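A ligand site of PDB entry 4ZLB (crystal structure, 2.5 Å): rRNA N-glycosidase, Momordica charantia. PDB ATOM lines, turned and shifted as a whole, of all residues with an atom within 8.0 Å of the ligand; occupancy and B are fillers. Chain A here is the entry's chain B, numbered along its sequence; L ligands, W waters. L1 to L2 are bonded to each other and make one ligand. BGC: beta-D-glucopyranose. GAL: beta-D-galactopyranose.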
ATOM      1  N   VAL A  21      -1.408 -18.186  14.162  1.00  0.00           N
ATOM      2  CA  VAL A  21      -2.321 -17.059  14.240  1.00  0.00           C
ATOM      3  C   VAL A  21      -2.060 -16.164  13.024  1.00  0.00           C
ATOM      4  O   VAL A  21      -0.930 -15.712  12.807  1.00  0.00           O
ATOM      5  CB  VAL A  21      -2.118 -16.265  15.545  1.00  0.00           C
ATOM      6  CG1 VAL A  21      -3.061 -15.071  15.629  1.00  0.00           C
ATOM      7  CG2 VAL A  21      -2.325 -17.181  16.751  1.00  0.00           C
ATOM      8  N   ASP A  22      -3.125 -15.914  12.270  1.00  0.00           N
ATOM      9  CA  ASP A  22      -3.059 -15.391  10.901  1.00  0.00           C
ATOM     10  C   ASP A  22      -4.246 -14.457  10.689  1.00  0.00           C
ATOM     11  O   ASP A  22      -5.378 -14.857  10.936  1.00  0.00           O
ATOM     12  CB  ASP A  22      -3.154 -16.600   9.936  1.00  0.00           C
ATOM     13  CG  ASP A  22      -3.085 -16.226   8.464  1.00  0.00           C
ATOM     14  OD1 ASP A  22      -3.891 -15.385   8.006  1.00  0.00           O
ATOM     15  OD2 ASP A  22      -2.251 -16.813   7.734  1.00  0.00           O
ATOM     16  N   VAL A  23      -3.999 -13.213  10.263  1.00  0.00           N
ATOM     17  CA  VAL A  23      -5.111 -12.303   9.897  1.00  0.00           C
ATOM     18  C   VAL A  23      -5.554 -12.623   8.462  1.00  0.00           C
ATOM     19  O   VAL A  23      -4.729 -12.629   7.546  1.00  0.00           O
ATOM     20  CB  VAL A  23      -4.855 -10.789  10.157  1.00  0.00           C
ATOM     21  CG1 VAL A  23      -3.672 -10.246   9.378  1.00  0.00           C
ATOM     22  CG2 VAL A  23      -6.113  -9.954   9.891  1.00  0.00           C
ATOM     23  N   TYR A  24      -6.847 -12.890   8.312  1.00  0.00           N
ATOM     24  CA  TYR A  24      -7.431 -13.476   7.099  1.00  0.00           C
ATOM     25  C   TYR A  24      -7.156 -12.677   5.829  1.00  0.00           C
ATOM     26  O   TYR A  24      -7.642 -11.555   5.672  1.00  0.00           O
ATOM     27  CB  TYR A  24      -8.955 -13.634   7.289  1.00  0.00           C
ATOM     28  CG  TYR A  24      -9.657 -14.132   6.050  1.00  0.00           C
ATOM     29  CD1 TYR A  24      -9.403 -15.409   5.556  1.00  0.00           C
ATOM     30  CD2 TYR A  24     -10.575 -13.325   5.361  1.00  0.00           C
ATOM     31  CE1 TYR A  24     -10.035 -15.871   4.402  1.00  0.00           C
ATOM     32  CE2 TYR A  24     -11.208 -13.779   4.213  1.00  0.00           C
ATOM     33  CZ  TYR A  24     -10.935 -15.050   3.748  1.00  0.00           C
ATOM     34  OH  TYR A  24     -11.568 -15.513   2.612  1.00  0.00           O
ATOM     35  N   GLY A  25      -6.370 -13.266   4.923  1.00  0.00           N
ATOM     36  CA  GLY A  25      -6.019 -12.659   3.639  1.00  0.00           C
ATOM     37  C   GLY A  25      -5.296 -11.323   3.719  1.00  0.00           C
ATOM     38  O   GLY A  25      -5.412 -10.510   2.813  1.00  0.00           O
ATOM     39  N   ALA A  26      -4.549 -11.120   4.807  1.00  0.00           N
ATOM     40  CA  ALA A  26      -3.778  -9.889   5.053  1.00  0.00           C
ATOM     41  C   ALA A  26      -4.595  -8.583   5.048  1.00  0.00           C
ATOM     42  O   ALA A  26      -4.046  -7.524   4.752  1.00  0.00           O
ATOM     43  CB  ALA A  26      -2.618  -9.801   4.052  1.00  0.00           C
ATOM     44  N   LEU A  27      -5.875  -8.659   5.419  1.00  0.00           N
ATOM     45  CA  LEU A  27      -6.768  -7.500   5.308  1.00  0.00           C
ATOM     46  C   LEU A  27      -6.414  -6.379   6.312  1.00  0.00           C
ATOM     47  O   LEU A  27      -6.206  -6.622   7.488  1.00  0.00           O
ATOM     48  CB  LEU A  27      -8.236  -7.917   5.470  1.00  0.00           C
ATOM     49  CG  LEU A  27      -8.806  -8.813   4.352  1.00  0.00           C
ATOM     50  CD1 LEU A  27     -10.098  -9.486   4.792  1.00  0.00           C
ATOM     51  CD2 LEU A  27      -9.026  -8.037   3.053  1.00  0.00           C
ATOM     52  N   ARG A  33     -10.808 -10.036  10.907  1.00  0.00           N
ATOM     53  CA  ARG A  33     -10.691 -11.187  11.809  1.00  0.00           C
ATOM     54  C   ARG A  33      -9.364 -11.918  11.699  1.00  0.00           C
ATOM     55  O   ARG A  33      -8.622 -11.757  10.726  1.00  0.00           O
ATOM     56  CB  ARG A  33     -11.844 -12.184  11.586  1.00  0.00           C
ATOM     57  CG  ARG A  33     -11.751 -13.010  10.305  1.00  0.00           C
ATOM     58  CD  ARG A  33     -12.915 -13.979  10.228  1.00  0.00           C
ATOM     59  NE  ARG A  33     -12.759 -14.917   9.108  1.00  0.00           N
ATOM     60  CZ  ARG A  33     -13.022 -14.644   7.832  1.00  0.00           C
ATOM     61  NH1 ARG A  33     -13.457 -13.440   7.443  1.00  0.00           N
ATOM     62  NH2 ARG A  33     -12.831 -15.598   6.910  1.00  0.00           N
ATOM     63  N   ILE A  35      -7.475 -15.882  12.253  1.00  0.00           N
ATOM     64  CA  ILE A  35      -7.797 -17.303  12.056  1.00  0.00           C
ATOM     65  C   ILE A  35      -6.615 -18.231  12.362  1.00  0.00           C
ATOM     66  O   ILE A  35      -5.493 -17.765  12.561  1.00  0.00           O
ATOM     67  CB  ILE A  35      -8.265 -17.580  10.592  1.00  0.00           C
ATOM     68  CG1 ILE A  35      -7.248 -17.041   9.580  1.00  0.00           C
ATOM     69  CG2 ILE A  35      -9.624 -16.956  10.333  1.00  0.00           C
ATOM     70  CD1 ILE A  35      -7.308 -17.700   8.211  1.00  0.00           C
ATOM     71  N   LEU A  36      -6.876 -19.534  12.374  1.00  0.00           N
ATOM     72  CA  LEU A  36      -5.812 -20.546  12.261  1.00  0.00           C
ATOM     73  C   LEU A  36      -5.417 -20.653  10.796  1.00  0.00           C
ATOM     74  O   LEU A  36      -6.282 -20.625   9.912  1.00  0.00           O
ATOM     75  CB  LEU A  36      -6.267 -21.922  12.765  1.00  0.00           C
ATOM     76  CG  LEU A  36      -6.423 -22.139  14.278  1.00  0.00           C
ATOM     77  CD1 LEU A  36      -7.085 -23.488  14.565  1.00  0.00           C
ATOM     78  CD2 LEU A  36      -5.079 -22.035  14.974  1.00  0.00           C
ATOM     79  N   TYR A  37      -4.112 -20.762  10.541  1.00  0.00           N
ATOM     80  CA  TYR A  37      -3.608 -20.989   9.193  1.00  0.00           C
ATOM     81  C   TYR A  37      -2.286 -21.741   9.244  1.00  0.00           C
ATOM     82  O   TYR A  37      -1.529 -21.567  10.204  1.00  0.00           O
ATOM     83  CB  TYR A  37      -3.443 -19.658   8.466  1.00  0.00           C
ATOM     84  CG  TYR A  37      -3.420 -19.800   6.965  1.00  0.00           C
ATOM     85  CD1 TYR A  37      -4.583 -20.141   6.270  1.00  0.00           C
ATOM     86  CD2 TYR A  37      -2.240 -19.634   6.233  1.00  0.00           C
ATOM     87  CE1 TYR A  37      -4.578 -20.297   4.884  1.00  0.00           C
ATOM     88  CE2 TYR A  37      -2.222 -19.788   4.848  1.00  0.00           C
ATOM     89  CZ  TYR A  37      -3.396 -20.110   4.176  1.00  0.00           C
ATOM     90  OH  TYR A  37      -3.392 -20.266   2.807  1.00  0.00           O
ATOM     91  N   PRO A  38      -2.009 -22.604   8.237  1.00  0.00           N
ATOM     92  CA  PRO A  38      -0.697 -23.256   8.221  1.00  0.00           C
ATOM     93  C   PRO A  38       0.444 -22.243   8.218  1.00  0.00           C
ATOM     94  O   PRO A  38       0.374 -21.215   7.540  1.00  0.00           O
ATOM     95  CB  PRO A  38      -0.720 -24.065   6.924  1.00  0.00           C
ATOM     96  CG  PRO A  38      -2.157 -24.345   6.692  1.00  0.00           C
ATOM     97  CD  PRO A  38      -2.868 -23.106   7.153  1.00  0.00           C
ATOM     98  N   GLY A  40       3.779 -19.992   7.961  1.00  0.00           N
ATOM     99  CA  GLY A  40       4.681 -19.540   6.890  1.00  0.00           C
ATOM    100  C   GLY A  40       5.343 -18.215   7.238  1.00  0.00           C
ATOM    101  O   GLY A  40       5.126 -17.680   8.325  1.00  0.00           O
ATOM    102  N   GLN A  42       4.912 -15.171   5.897  1.00  0.00           N
ATOM    103  CA  GLN A  42       4.171 -13.996   5.412  1.00  0.00           C
ATOM    104  C   GLN A  42       3.980 -12.935   6.493  1.00  0.00           C
ATOM    105  O   GLN A  42       3.953 -13.242   7.668  1.00  0.00           O
ATOM    106  CB  GLN A  42       2.810 -14.389   4.810  1.00  0.00           C
ATOM    107  CG  GLN A  42       1.897 -15.241   5.691  1.00  0.00           C
ATOM    108  CD  GLN A  42       1.920 -16.712   5.318  1.00  0.00           C
ATOM    109  OE1 GLN A  42       2.984 -17.271   5.039  1.00  0.00           O
ATOM    110  NE2 GLN A  42       0.752 -17.346   5.331  1.00  0.00           N
ATOM    111  N   GLN A  43       3.835 -11.687   6.044  1.00  0.00           N
ATOM    112  CA  GLN A  43       3.846 -10.517   6.941  1.00  0.00           C
ATOM    113  C   GLN A  43       2.671 -10.482   7.910  1.00  0.00           C
ATOM    114  O   GLN A  43       2.781  -9.938   9.007  1.00  0.00           O
ATOM    115  CB  GLN A  43       3.875  -9.209   6.131  1.00  0.00           C
ATOM    116  CG  GLN A  43       5.120  -9.002   5.276  1.00  0.00           C
ATOM    117  CD  GLN A  43       6.359  -8.700   6.106  1.00  0.00           C
ATOM    118  OE1 GLN A  43       7.288  -9.512   6.183  1.00  0.00           O
ATOM    119  NE2 GLN A  43       6.368  -7.524   6.743  1.00  0.00           N
ATOM    120  N   ASN A  44       1.547 -11.067   7.499  1.00  0.00           N
ATOM    121  CA  ASN A  44       0.325 -11.097   8.308  1.00  0.00           C
ATOM    122  C   ASN A  44       0.270 -12.209   9.388  1.00  0.00           C
ATOM    123  O   ASN A  44      -0.711 -12.304  10.120  1.00  0.00           O
ATOM    124  CB  ASN A  44      -0.913 -11.158   7.393  1.00  0.00           C
ATOM    125  CG  ASN A  44      -0.986 -12.437   6.576  1.00  0.00           C
ATOM    126  OD1 ASN A  44      -0.059 -12.739   5.824  1.00  0.00           O
ATOM    127  ND2 ASN A  44      -2.090 -13.172   6.705  1.00  0.00           N
ATOM    128  N   GLN A  45       1.310 -13.052   9.464  1.00  0.00           N
ATOM    129  CA  GLN A  45       1.542 -13.971  10.604  1.00  0.00           C
ATOM    130  C   GLN A  45       2.655 -13.454  11.556  1.00  0.00           C
ATOM    131  O   GLN A  45       2.994 -14.141  12.529  1.00  0.00           O
ATOM    132  CB  GLN A  45       1.914 -15.389  10.105  1.00  0.00           C
ATOM    133  CG  GLN A  45       0.732 -16.258   9.723  1.00  0.00           C
ATOM    134  CD  GLN A  45       1.142 -17.665   9.284  1.00  0.00           C
ATOM    135  OE1 GLN A  45       2.287 -18.089   9.463  1.00  0.00           O
ATOM    136  NE2 GLN A  45       0.195 -18.400   8.709  1.00  0.00           N
ATOM    137  N   SER A 111      -7.946 -25.290   9.099  1.00  0.00           N
ATOM    138  CA  SER A 111      -7.544 -24.017   8.485  1.00  0.00           C
ATOM    139  C   SER A 111      -8.730 -23.046   8.308  1.00  0.00           C
ATOM    140  O   SER A 111      -9.875 -23.477   8.190  1.00  0.00           O
ATOM    141  CB  SER A 111      -6.874 -24.243   7.122  1.00  0.00           C
ATOM    142  OG  SER A 111      -6.301 -23.061   6.617  1.00  0.00           O
ATOM    143  N   ARG A 112      -8.441 -21.749   8.326  1.00  0.00           N
ATOM    144  CA  ARG A 112      -9.462 -20.687   8.298  1.00  0.00           C
ATOM    145  C   ARG A 112     -10.458 -20.675   9.472  1.00  0.00           C
ATOM    146  O   ARG A 112     -11.508 -20.019   9.373  1.00  0.00           O
ATOM    147  CB  ARG A 112     -10.249 -20.708   6.977  1.00  0.00           C
ATOM    148  CG  ARG A 112      -9.412 -20.557   5.720  1.00  0.00           C
ATOM    149  CD  ARG A 112     -10.299 -20.049   4.595  1.00  0.00           C
ATOM    150  NE  ARG A 112      -9.753 -20.334   3.282  1.00  0.00           N
ATOM    151  CZ  ARG A 112     -10.357 -20.072   2.128  1.00  0.00           C
ATOM    152  NH1 ARG A 112     -11.559 -19.486   2.107  1.00  0.00           N
ATOM    153  NH2 ARG A 112      -9.758 -20.387   0.984  1.00  0.00           N
HETATM  154  C2  BGC L   1      -7.150 -13.959  -1.044  1.00  0.00           C
HETATM  155  C3  BGC L   1      -6.375 -14.267   0.227  1.00  0.00           C
HETATM  156  C4  BGC L   1      -4.862 -14.394  -0.007  1.00  0.00           C
HETATM  157  C5  BGC L   1      -4.330 -13.282  -0.932  1.00  0.00           C
HETATM  158  C6  BGC L   1      -2.885 -13.542  -1.323  1.00  0.00           C
HETATM  159  C1  BGC L   1      -6.499 -12.790  -1.782  1.00  0.00           C
HETATM  160  O1  BGC L   1      -7.228 -12.482  -2.975  1.00  0.00           O
HETATM  161  O2  BGC L   1      -8.522 -13.688  -0.701  1.00  0.00           O
HETATM  162  O3  BGC L   1      -6.891 -15.503   0.732  1.00  0.00           O
HETATM  163  O4  BGC L   1      -4.138 -14.288   1.221  1.00  0.00           O
HETATM  164  O5  BGC L   1      -5.144 -13.154  -2.105  1.00  0.00           O
HETATM  165  O6  BGC L   1      -2.709 -14.861  -1.863  1.00  0.00           O
HETATM  166  C1  GAL L   2      -3.935 -15.499   1.970  1.00  0.00           C
HETATM  167  C2  GAL L   2      -2.779 -15.269   2.944  1.00  0.00           C
HETATM  168  C3  GAL L   2      -2.753 -16.257   4.113  1.00  0.00           C
HETATM  169  C4  GAL L   2      -4.149 -16.510   4.693  1.00  0.00           C
HETATM  170  C5  GAL L   2      -5.075 -16.912   3.562  1.00  0.00           C
HETATM  171  C6  GAL L   2      -6.481 -17.271   4.047  1.00  0.00           C
HETATM  172  O2  GAL L   2      -1.524 -15.365   2.242  1.00  0.00           O
HETATM  173  O3  GAL L   2      -1.844 -15.788   5.118  1.00  0.00           O
HETATM  174  O4  GAL L   2      -4.669 -15.337   5.352  1.00  0.00           O
HETATM  175  O5  GAL L   2      -5.158 -15.806   2.661  1.00  0.00           O
HETATM  176  O6  GAL L   2      -7.248 -17.756   2.944  1.00  0.00           O
HETATM  177  O   HOH W   1      -9.473 -16.679   1.421  1.00  0.00           O
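Water W1 bridges the side-chain hydroxyl of Tyr 24 (2.7 Å) and an oxygen (O6) of GAL L2 (2.9 Å).
OD1 of Asp 22 is in hydrogen-bond range of ND2 of Asn 44 (3.1 Å). The backbone carbonyl oxygen of Asp 22 sits at hydrogen-bond distance from the backbone NH of Ile 35 (2.7 Å). The side-chain carboxylate of Asp 22 is in hydrogen-bond range of the side-chain amide nitrogen of Gln 45. ND2 of Asn 44 sits at hydrogen-bond distance from O of Val 23 (2.8 Å). The backbone carbonyl oxygen of Leu 36 is in hydrogen-bond range of the backbone NH of Arg 112, 2.9 Å away. N of Tyr 24 sits at hydrogen-bond distance from O of Arg 33.
N of Gly 25 is in hydrogen-bond range of O4 of GAL L2 (2.7 Å). The side-chain carboxylate of Asp 22 lies within hydrogen-bond range of an oxygen (O4) of GAL L2. NE2 of Gln 42 lies within hydrogen-bond range of O3 of GAL L2 (3.0 Å). An oxygen (O3) of GAL L2 lies within hydrogen-bond range of the side-chain amide nitrogen (ND2) of Asn 44, 3.1 Å away. An oxygen (O4) of GAL L2 sits at hydrogen-bond distance from the backbone carbonyl oxygen of Val 23.
Merely in contact with the ligand: Arg 112 (3.6 Å), Tyr 37 (3.6 Å) and Tyr 24 (3.7 Å). Of the 19 residues printed, 8 come within 4 Å of the ligand. The nearest printed residue that does not touch the ligand is Ala 26 (4.3 Å).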
